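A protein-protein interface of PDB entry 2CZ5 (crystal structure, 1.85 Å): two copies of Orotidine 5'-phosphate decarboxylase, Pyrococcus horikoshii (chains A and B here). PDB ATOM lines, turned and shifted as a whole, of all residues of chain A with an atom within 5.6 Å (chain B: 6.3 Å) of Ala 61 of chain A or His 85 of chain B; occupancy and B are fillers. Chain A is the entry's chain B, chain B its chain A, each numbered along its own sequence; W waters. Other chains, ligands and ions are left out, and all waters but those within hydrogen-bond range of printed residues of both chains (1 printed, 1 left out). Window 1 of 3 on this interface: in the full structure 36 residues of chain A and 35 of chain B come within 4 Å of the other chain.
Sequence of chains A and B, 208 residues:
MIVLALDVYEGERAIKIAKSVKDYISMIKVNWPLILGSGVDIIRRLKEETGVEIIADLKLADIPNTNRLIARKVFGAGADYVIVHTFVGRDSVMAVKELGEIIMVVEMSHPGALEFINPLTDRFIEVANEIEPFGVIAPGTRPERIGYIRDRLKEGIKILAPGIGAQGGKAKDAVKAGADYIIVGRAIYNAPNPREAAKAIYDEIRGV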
ATOM      1  N   LYS A  59     -16.467   9.078 -29.542  1.00  0.00           N
ATOM      2  CA  LYS A  59     -17.829   8.779 -29.104  1.00  0.00           C
ATOM      3  C   LYS A  59     -18.782   8.785 -30.316  1.00  0.00           C
ATOM      4  O   LYS A  59     -19.892   9.330 -30.226  1.00  0.00           O
ATOM      5  CB  LYS A  59     -18.305   9.850 -28.097  1.00  0.00           C
ATOM      6  CG  LYS A  59     -17.450  10.032 -26.821  1.00  0.00           C
ATOM      7  CD  LYS A  59     -17.614   8.877 -25.839  1.00  0.00           C
ATOM      8  CE  LYS A  59     -16.921   9.116 -24.475  1.00  0.00           C
ATOM      9  NZ  LYS A  59     -15.525   9.694 -24.529  1.00  0.00           N
ATOM     10  N   LEU A  60     -18.368   8.194 -31.446  1.00  0.00           N
ATOM     11  CA  LEU A  60     -19.244   8.195 -32.625  1.00  0.00           C
ATOM     12  C   LEU A  60     -20.637   7.674 -32.290  1.00  0.00           C
ATOM     13  O   LEU A  60     -20.796   6.634 -31.642  1.00  0.00           O
ATOM     14  CB  LEU A  60     -18.639   7.381 -33.779  1.00  0.00           C
ATOM     15  CG  LEU A  60     -17.309   7.926 -34.322  1.00  0.00           C
ATOM     16  CD1 LEU A  60     -16.923   7.130 -35.568  1.00  0.00           C
ATOM     17  CD2 LEU A  60     -17.432   9.422 -34.673  1.00  0.00           C
ATOM     18  N   ALA A  61     -21.650   8.392 -32.764  1.00  0.00           N
ATOM     19  CA  ALA A  61     -23.021   8.037 -32.456  1.00  0.00           C
ATOM     20  C   ALA A  61     -23.973   8.556 -33.521  1.00  0.00           C
ATOM     21  O   ALA A  61     -24.992   9.211 -33.204  1.00  0.00           O
ATOM     22  CB  ALA A  61     -23.399   8.629 -31.105  1.00  0.00           C
ATOM     23  N   ASP A  62     -23.633   8.297 -34.774  1.00  0.00           N
ATOM     24  CA  ASP A  62     -24.470   8.731 -35.884  1.00  0.00           C
ATOM     25  C   ASP A  62     -24.931   7.507 -36.674  1.00  0.00           C
ATOM     26  O   ASP A  62     -24.613   6.374 -36.293  1.00  0.00           O
ATOM     27  CB  ASP A  62     -23.700   9.725 -36.759  1.00  0.00           C
ATOM     28  CG  ASP A  62     -24.607  10.794 -37.362  1.00  0.00           C
ATOM     29  OD1 ASP A  62     -25.631  10.409 -37.970  1.00  0.00           O
ATOM     30  OD2 ASP A  62     -24.297  12.008 -37.241  1.00  0.00           O
ATOM     31  N   ILE A  63     -25.693   7.719 -37.753  1.00  0.00           N
ATOM     32  CA  ILE A  63     -26.186   6.616 -38.566  1.00  0.00           C
ATOM     33  C   ILE A  63     -24.973   5.956 -39.246  1.00  0.00           C
ATOM     34  O   ILE A  63     -23.902   6.552 -39.324  1.00  0.00           O
ATOM     35  CB  ILE A  63     -27.176   7.117 -39.649  1.00  0.00           C
ATOM     36  CG1 ILE A  63     -26.467   8.116 -40.569  1.00  0.00           C
ATOM     37  CG2 ILE A  63     -28.387   7.818 -38.974  1.00  0.00           C
ATOM     38  CD1 ILE A  63     -27.271   8.508 -41.814  1.00  0.00           C
ATOM     39  N   ASN A  67     -21.204   7.688 -39.759  1.00  0.00           N
ATOM     40  CA  ASN A  67     -20.141   7.136 -38.908  1.00  0.00           C
ATOM     41  C   ASN A  67     -19.038   6.660 -39.861  1.00  0.00           C
ATOM     42  O   ASN A  67     -17.853   6.767 -39.567  1.00  0.00           O
ATOM     43  CB  ASN A  67     -20.635   5.909 -38.124  1.00  0.00           C
ATOM     44  CG  ASN A  67     -21.127   6.250 -36.722  1.00  0.00           C
ATOM     45  OD1 ASN A  67     -21.377   7.409 -36.407  1.00  0.00           O
ATOM     46  ND2 ASN A  67     -21.282   5.223 -35.878  1.00  0.00           N
ATOM     47  N   HIS A  85     -19.854   4.808 -29.534  1.00  0.00           N
ATOM     48  CA  HIS A  85     -20.931   4.440 -28.628  1.00  0.00           C
ATOM     49  C   HIS A  85     -21.571   3.141 -29.111  1.00  0.00           C
ATOM     50  O   HIS A  85     -21.520   2.797 -30.308  1.00  0.00           O
ATOM     51  CB  HIS A  85     -22.005   5.537 -28.555  1.00  0.00           C
ATOM     52  CG  HIS A  85     -21.780   6.501 -27.444  1.00  0.00           C
ATOM     53  ND1 HIS A  85     -21.705   6.104 -26.125  1.00  0.00           N
ATOM     54  CD2 HIS A  85     -21.542   7.834 -27.453  1.00  0.00           C
ATOM     55  CE1 HIS A  85     -21.426   7.148 -25.371  1.00  0.00           C
ATOM     56  NE2 HIS A  85     -21.320   8.211 -26.151  1.00  0.00           N
ATOM     57  N   PHE A  87     -24.816   2.474 -27.898  1.00  0.00           N
ATOM     58  CA  PHE A  87     -26.249   2.760 -27.942  1.00  0.00           C
ATOM     59  C   PHE A  87     -26.904   3.097 -29.282  1.00  0.00           C
ATOM     60  O   PHE A  87     -28.124   2.960 -29.416  1.00  0.00           O
ATOM     61  CB  PHE A  87     -26.603   3.825 -26.897  1.00  0.00           C
ATOM     62  CG  PHE A  87     -26.273   5.233 -27.292  1.00  0.00           C
ATOM     63  CD1 PHE A  87     -27.121   5.950 -28.133  1.00  0.00           C
ATOM     64  CD2 PHE A  87     -25.187   5.888 -26.720  1.00  0.00           C
ATOM     65  CE1 PHE A  87     -26.904   7.312 -28.386  1.00  0.00           C
ATOM     66  CE2 PHE A  87     -24.956   7.252 -26.969  1.00  0.00           C
ATOM     67  CZ  PHE A  87     -25.825   7.964 -27.804  1.00  0.00           C
ATOM     68  N   VAL A  88     -26.117   3.506 -30.277  1.00  0.00           N
ATOM     69  CA  VAL A  88     -26.697   3.842 -31.571  1.00  0.00           C
ATOM     70  C   VAL A  88     -27.021   2.617 -32.423  1.00  0.00           C
ATOM     71  O   VAL A  88     -27.642   2.730 -33.482  1.00  0.00           O
ATOM     72  CB  VAL A  88     -25.801   4.864 -32.329  1.00  0.00           C
ATOM     73  CG1 VAL A  88     -26.317   5.105 -33.723  1.00  0.00           C
ATOM     74  CG2 VAL A  88     -25.815   6.189 -31.583  1.00  0.00           C
ATOM     75  N   LEU B  58     -23.206  17.463 -34.249  1.00  0.00           N
ATOM     76  CA  LEU B  58     -22.112  16.777 -33.614  1.00  0.00           C
ATOM     77  C   LEU B  58     -22.493  15.524 -32.839  1.00  0.00           C
ATOM     78  O   LEU B  58     -21.602  14.801 -32.391  1.00  0.00           O
ATOM     79  CB  LEU B  58     -21.391  17.762 -32.693  1.00  0.00           C
ATOM     80  CG  LEU B  58     -20.992  19.091 -33.353  1.00  0.00           C
ATOM     81  CD1 LEU B  58     -20.329  19.974 -32.313  1.00  0.00           C
ATOM     82  CD2 LEU B  58     -20.027  18.826 -34.544  1.00  0.00           C
ATOM     83  N   LYS B  59     -23.802  15.269 -32.693  1.00  0.00           N
ATOM     84  CA  LYS B  59     -24.297  14.111 -31.942  1.00  0.00           C
ATOM     85  C   LYS B  59     -23.525  14.055 -30.623  1.00  0.00           C
ATOM     86  O   LYS B  59     -23.025  12.989 -30.238  1.00  0.00           O
ATOM     87  CB  LYS B  59     -24.059  12.804 -32.715  1.00  0.00           C
ATOM     88  CG  LYS B  59     -24.742  12.683 -34.079  1.00  0.00           C
ATOM     89  CD  LYS B  59     -26.263  12.752 -33.966  1.00  0.00           C
ATOM     90  CE  LYS B  59     -26.962  12.290 -35.252  1.00  0.00           C
ATOM     91  NZ  LYS B  59     -26.544  13.070 -36.441  1.00  0.00           N
ATOM     92  N   LEU B  60     -23.420  15.187 -29.926  1.00  0.00           N
ATOM     93  CA  LEU B  60     -22.640  15.204 -28.674  1.00  0.00           C
ATOM     94  C   LEU B  60     -23.164  14.156 -27.701  1.00  0.00           C
ATOM     95  O   LEU B  60     -24.373  14.079 -27.407  1.00  0.00           O
ATOM     96  CB  LEU B  60     -22.615  16.611 -28.045  1.00  0.00           C
ATOM     97  CG  LEU B  60     -21.921  17.717 -28.863  1.00  0.00           C
ATOM     98  CD1 LEU B  60     -21.733  18.938 -27.985  1.00  0.00           C
ATOM     99  CD2 LEU B  60     -20.546  17.247 -29.382  1.00  0.00           C
ATOM    100  N   ALA B  61     -22.234  13.346 -27.205  1.00  0.00           N
ATOM    101  CA  ALA B  61     -22.567  12.240 -26.321  1.00  0.00           C
ATOM    102  C   ALA B  61     -21.445  11.938 -25.323  1.00  0.00           C
ATOM    103  O   ALA B  61     -21.069  10.779 -25.131  1.00  0.00           O
ATOM    104  CB  ALA B  61     -22.860  10.995 -27.171  1.00  0.00           C
ATOM    105  N   ASN B  67     -18.440  17.812 -23.237  1.00  0.00           N
ATOM    106  CA  ASN B  67     -19.488  18.413 -24.078  1.00  0.00           C
ATOM    107  C   ASN B  67     -19.340  19.949 -24.040  1.00  0.00           C
ATOM    108  O   ASN B  67     -19.485  20.617 -25.057  1.00  0.00           O
ATOM    109  CB  ASN B  67     -20.896  18.057 -23.559  1.00  0.00           C
ATOM    110  CG  ASN B  67     -21.460  16.788 -24.177  1.00  0.00           C
ATOM    111  OD1 ASN B  67     -20.729  16.001 -24.797  1.00  0.00           O
ATOM    112  ND2 ASN B  67     -22.768  16.574 -24.003  1.00  0.00           N
ATOM    113  N   ILE B  83     -26.336  19.942 -32.222  1.00  0.00           N
ATOM    114  CA  ILE B  83     -27.168  18.772 -32.008  1.00  0.00           C
ATOM    115  C   ILE B  83     -26.518  17.872 -30.971  1.00  0.00           C
ATOM    116  O   ILE B  83     -25.325  17.539 -31.074  1.00  0.00           O
ATOM    117  CB  ILE B  83     -27.397  18.008 -33.309  1.00  0.00           C
ATOM    118  CG1 ILE B  83     -28.282  18.852 -34.238  1.00  0.00           C
ATOM    119  CG2 ILE B  83     -28.036  16.653 -33.018  1.00  0.00           C
ATOM    120  CD1 ILE B  83     -28.436  18.282 -35.644  1.00  0.00           C
ATOM    121  N   VAL B  84     -27.310  17.488 -29.967  1.00  0.00           N
ATOM    122  CA  VAL B  84     -26.842  16.632 -28.886  1.00  0.00           C
ATOM    123  C   VAL B  84     -27.752  15.416 -28.717  1.00  0.00           C
ATOM    124  O   VAL B  84     -28.933  15.447 -29.076  1.00  0.00           O
ATOM    125  CB  VAL B  84     -26.784  17.422 -27.536  1.00  0.00           C
ATOM    126  CG1 VAL B  84     -26.052  18.737 -27.753  1.00  0.00           C
ATOM    127  CG2 VAL B  84     -28.201  17.692 -26.992  1.00  0.00           C
ATOM    128  N   HIS B  85     -27.197  14.329 -28.205  1.00  0.00           N
ATOM    129  CA  HIS B  85     -27.996  13.129 -27.964  1.00  0.00           C
ATOM    130  C   HIS B  85     -28.662  13.268 -26.599  1.00  0.00           C
ATOM    131  O   HIS B  85     -28.081  13.843 -25.684  1.00  0.00           O
ATOM    132  CB  HIS B  85     -27.124  11.882 -27.934  1.00  0.00           C
ATOM    133  CG  HIS B  85     -27.027  11.172 -29.249  1.00  0.00           C
ATOM    134  ND1 HIS B  85     -28.103  10.538 -29.835  1.00  0.00           N
ATOM    135  CD2 HIS B  85     -25.966  10.942 -30.061  1.00  0.00           C
ATOM    136  CE1 HIS B  85     -27.708   9.942 -30.947  1.00  0.00           C
ATOM    137  NE2 HIS B  85     -26.415  10.171 -31.107  1.00  0.00           N
ATOM    138  N   THR B  86     -29.869  12.736 -26.456  1.00  0.00           N
ATOM    139  CA  THR B  86     -30.562  12.795 -25.167  1.00  0.00           C
ATOM    140  C   THR B  86     -30.080  11.636 -24.282  1.00  0.00           C
ATOM    141  O   THR B  86     -30.049  11.742 -23.057  1.00  0.00           O
ATOM    142  CB  THR B  86     -32.088  12.654 -25.344  1.00  0.00           C
ATOM    143  OG1 THR B  86     -32.554  13.621 -26.296  1.00  0.00           O
ATOM    144  CG2 THR B  86     -32.794  12.859 -24.025  1.00  0.00           C
ATOM    145  N   PHE B  87     -29.662  10.553 -24.939  1.00  0.00           N
ATOM    146  CA  PHE B  87     -29.213   9.315 -24.308  1.00  0.00           C
ATOM    147  C   PHE B  87     -28.149   9.412 -23.209  1.00  0.00           C
ATOM    148  O   PHE B  87     -28.191   8.664 -22.235  1.00  0.00           O
ATOM    149  CB  PHE B  87     -28.703   8.373 -25.397  1.00  0.00           C
ATOM    150  CG  PHE B  87     -29.035   6.938 -25.164  1.00  0.00           C
ATOM    151  CD1 PHE B  87     -28.550   6.259 -24.041  1.00  0.00           C
ATOM    152  CD2 PHE B  87     -29.837   6.256 -26.063  1.00  0.00           C
ATOM    153  CE1 PHE B  87     -28.870   4.916 -23.822  1.00  0.00           C
ATOM    154  CE2 PHE B  87     -30.161   4.907 -25.850  1.00  0.00           C
ATOM    155  CZ  PHE B  87     -29.677   4.246 -24.728  1.00  0.00           C
ATOM    156  N   VAL B  88     -27.213  10.340 -23.346  1.00  0.00           N
ATOM    157  CA  VAL B  88     -26.146  10.452 -22.361  1.00  0.00           C
ATOM    158  C   VAL B  88     -26.540  11.175 -21.063  1.00  0.00           C
ATOM    159  O   VAL B  88     -25.746  11.276 -20.129  1.00  0.00           O
ATOM    160  CB  VAL B  88     -24.905  11.080 -23.026  1.00  0.00           C
ATOM    161  CG1 VAL B  88     -23.785  11.296 -22.024  1.00  0.00           C
ATOM    162  CG2 VAL B  88     -24.414  10.121 -24.116  1.00  0.00           C
ATOM    163  N   GLY B  89     -27.766  11.675 -21.003  1.00  0.00           N
ATOM    164  CA  GLY B  89     -28.194  12.306 -19.761  1.00  0.00           C
ATOM    165  C   GLY B  89     -28.465  13.790 -19.789  1.00  0.00           C
ATOM    166  O   GLY B  89     -27.927  14.528 -20.604  1.00  0.00           O
ATOM    167  N   SER B  92     -25.335  16.301 -19.392  1.00  0.00           N
ATOM    168  CA  SER B  92     -24.546  16.499 -20.599  1.00  0.00           C
ATOM    169  C   SER B  92     -25.265  17.401 -21.603  1.00  0.00           C
ATOM    170  O   SER B  92     -24.630  18.123 -22.380  1.00  0.00           O
ATOM    171  CB  SER B  92     -24.227  15.151 -21.244  1.00  0.00           C
ATOM    172  OG  SER B  92     -23.367  14.427 -20.399  1.00  0.00           O
ATOM    173  N   VAL B  93     -26.593  17.374 -21.582  1.00  0.00           N
ATOM    174  CA  VAL B  93     -27.369  18.210 -22.491  1.00  0.00           C
ATOM    175  C   VAL B  93     -27.307  19.673 -22.038  1.00  0.00           C
ATOM    176  O   VAL B  93     -27.122  20.590 -22.859  1.00  0.00           O
ATOM    177  CB  VAL B  93     -28.849  17.728 -22.554  1.00  0.00           C
ATOM    178  CG1 VAL B  93     -29.730  18.750 -23.289  1.00  0.00           C
ATOM    179  CG2 VAL B  93     -28.920  16.388 -23.261  1.00  0.00           C
ATOM    180  N   ILE B 103     -30.478  21.226 -30.298  1.00  0.00           N
ATOM    181  CA  ILE B 103     -31.473  20.392 -30.932  1.00  0.00           C
ATOM    182  C   ILE B 103     -31.168  19.030 -30.330  1.00  0.00           C
ATOM    183  O   ILE B 103     -30.012  18.620 -30.271  1.00  0.00           O
ATOM    184  CB  ILE B 103     -31.289  20.358 -32.453  1.00  0.00           C
ATOM    185  CG1 ILE B 103     -31.706  21.706 -33.048  1.00  0.00           C
ATOM    186  CG2 ILE B 103     -32.063  19.195 -33.046  1.00  0.00           C
ATOM    187  CD1 ILE B 103     -31.093  22.000 -34.408  1.00  0.00           C
ATOM    188  N   MET B 104     -32.203  18.334 -29.887  1.00  0.00           N
ATOM    189  CA  MET B 104     -32.030  17.032 -29.254  1.00  0.00           C
ATOM    190  C   MET B 104     -32.452  15.833 -30.095  1.00  0.00           C
ATOM    191  O   MET B 104     -33.484  15.845 -30.758  1.00  0.00           O
ATOM    192  CB  MET B 104     -32.793  17.024 -27.921  1.00  0.00           C
ATOM    193  CG  MET B 104     -32.148  17.873 -26.835  1.00  0.00           C
ATOM    194  SD  MET B 104     -33.253  18.081 -25.364  1.00  0.00           S
ATOM    195  CE  MET B 104     -33.256  16.455 -24.722  1.00  0.00           C
ATOM    196  N   VAL B 105     -31.626  14.791 -30.088  1.00  0.00           N
ATOM    197  CA  VAL B 105     -31.971  13.585 -30.818  1.00  0.00           C
ATOM    198  C   VAL B 105     -32.910  12.749 -29.957  1.00  0.00           C
ATOM    199  O   VAL B 105     -32.539  12.323 -28.858  1.00  0.00           O
ATOM    200  CB  VAL B 105     -30.723  12.741 -31.127  1.00  0.00           C
ATOM    201  CG1 VAL B 105     -31.129  11.489 -31.881  1.00  0.00           C
ATOM    202  CG2 VAL B 105     -29.728  13.566 -31.904  1.00  0.00           C
ATOM    203  N   MET B 108     -34.125   7.886 -34.160  1.00  0.00           N
ATOM    204  CA  MET B 108     -33.302   7.818 -35.369  1.00  0.00           C
ATOM    205  C   MET B 108     -33.898   6.888 -36.424  1.00  0.00           C
ATOM    206  O   MET B 108     -34.778   6.092 -36.120  1.00  0.00           O
ATOM    207  CB  MET B 108     -31.865   7.430 -35.008  1.00  0.00           C
ATOM    208  CG  MET B 108     -31.167   8.537 -34.209  1.00  0.00           C
ATOM    209  SD  MET B 108     -29.429   8.234 -33.818  1.00  0.00           S
ATOM    210  CE  MET B 108     -28.668   8.775 -35.375  1.00  0.00           C
ATOM    211  N   ILE B 117     -32.222   3.257 -28.967  1.00  0.00           N
ATOM    212  CA  ILE B 117     -32.751   4.610 -29.058  1.00  0.00           C
ATOM    213  C   ILE B 117     -34.266   4.733 -29.158  1.00  0.00           C
ATOM    214  O   ILE B 117     -34.906   5.370 -28.312  1.00  0.00           O
ATOM    215  CB  ILE B 117     -32.122   5.360 -30.239  1.00  0.00           C
ATOM    216  CG1 ILE B 117     -30.612   5.495 -30.011  1.00  0.00           C
ATOM    217  CG2 ILE B 117     -32.772   6.726 -30.395  1.00  0.00           C
ATOM    218  CD1 ILE B 117     -29.875   6.182 -31.158  1.00  0.00           C
HETATM  219  O   HOH W   1     -30.479   2.242 -30.815  1.00  0.00           O
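Of chain B, only Lys 59 and His 85 come within 4 Å of Ala 61 of chain A. Of the printed residues of chain B, Phe 87 of chain A touches His 85 (3.7 Å), Phe 87 (3.4 Å) and Ile 117 (3.6 Å). Of the printed residues of chain A, Ala 61 of chain B touches His 85 (2.8 Å). Of chain A, only Ala 61 (2.7 Å) and Phe 87 (3.7 Å) come within 4 Å of His 85 of chain B.
Ala 61 of chain A touches Lys 59 of chain B, but with the chains exchanged Lys 59 of chain A does not touch Ala 61 of chain B (4.01 Å). Ala 61 of chain A touches His 85 of chain B, and with the chains exchanged His 85 of chain A touches Ala 61 of chain B. Phe 87 of chain A touches His 85 of chain B, but with the chains exchanged His 85 of chain A does not touch Phe 87 of chain B (7.2 Å). Phe 87 of chain A touches its own counterpart, Phe 87 of chain B. Of the 9 pairs that touch across the chains among the printed residues, 3 have their exchanged pair printed and touching as well.
Water W1 lies within hydrogen-bond range of the backbone NH of Ile 117 of chain B (2.7 Å) and the backbone carbonyl oxygen of Phe 87 of chain A (2.8 Å).
The backbone NH (N) of Lys 59 of chain B sits at hydrogen-bond distance from the backbone carbonyl oxygen (O) of Ile 83 of chain B, 3.2 Å away. N of His 85 of chain B lies within hydrogen-bond range of O of Leu 60 of chain B (2.9 Å). N of His 85 of chain A is in hydrogen-bond range of O of Leu 60 of chain A (2.9 Å). The side-chain amide oxygen (OD1) of Asn 67 of chain A is in hydrogen-bond range of the backbone NH (N) of Asp 62 of chain A (2.9 Å).
Among the printed residues, merely in contact across the chains: Ala 61 of chain A with Lys 59 of chain B (3.6 Å), Ile 63 of chain A with Met 108 of chain B (3.7 Å), Phe 87 of chain A with His 85 of chain B (3.7 Å), Phe 87 of chain A with Phe 87 of chain B (3.4 Å), Phe 87 of chain A with Ile 117 of chain B (3.6 Å) and Val 88 of chain A with Ile 117 of chain B (3.97 Å).
NZ of Lys 59 of chain B lies within salt-bridge range of OD2 of Asp 62 of chain A (2.6 Å). O of Ala 61 of chain B lies within hydrogen-bond range of NE2 of His 85 of chain A. The backbone carbonyl oxygen (O) of Ala 61 of chain A is in hydrogen-bond range of a ring nitrogen (NE2) of His 85 of chain B (2.7 Å).
Of the 9 printed residues of chain A, 6 touch a printed residue of chain B. Among the printed residues, 9 pairs touch across the chains.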
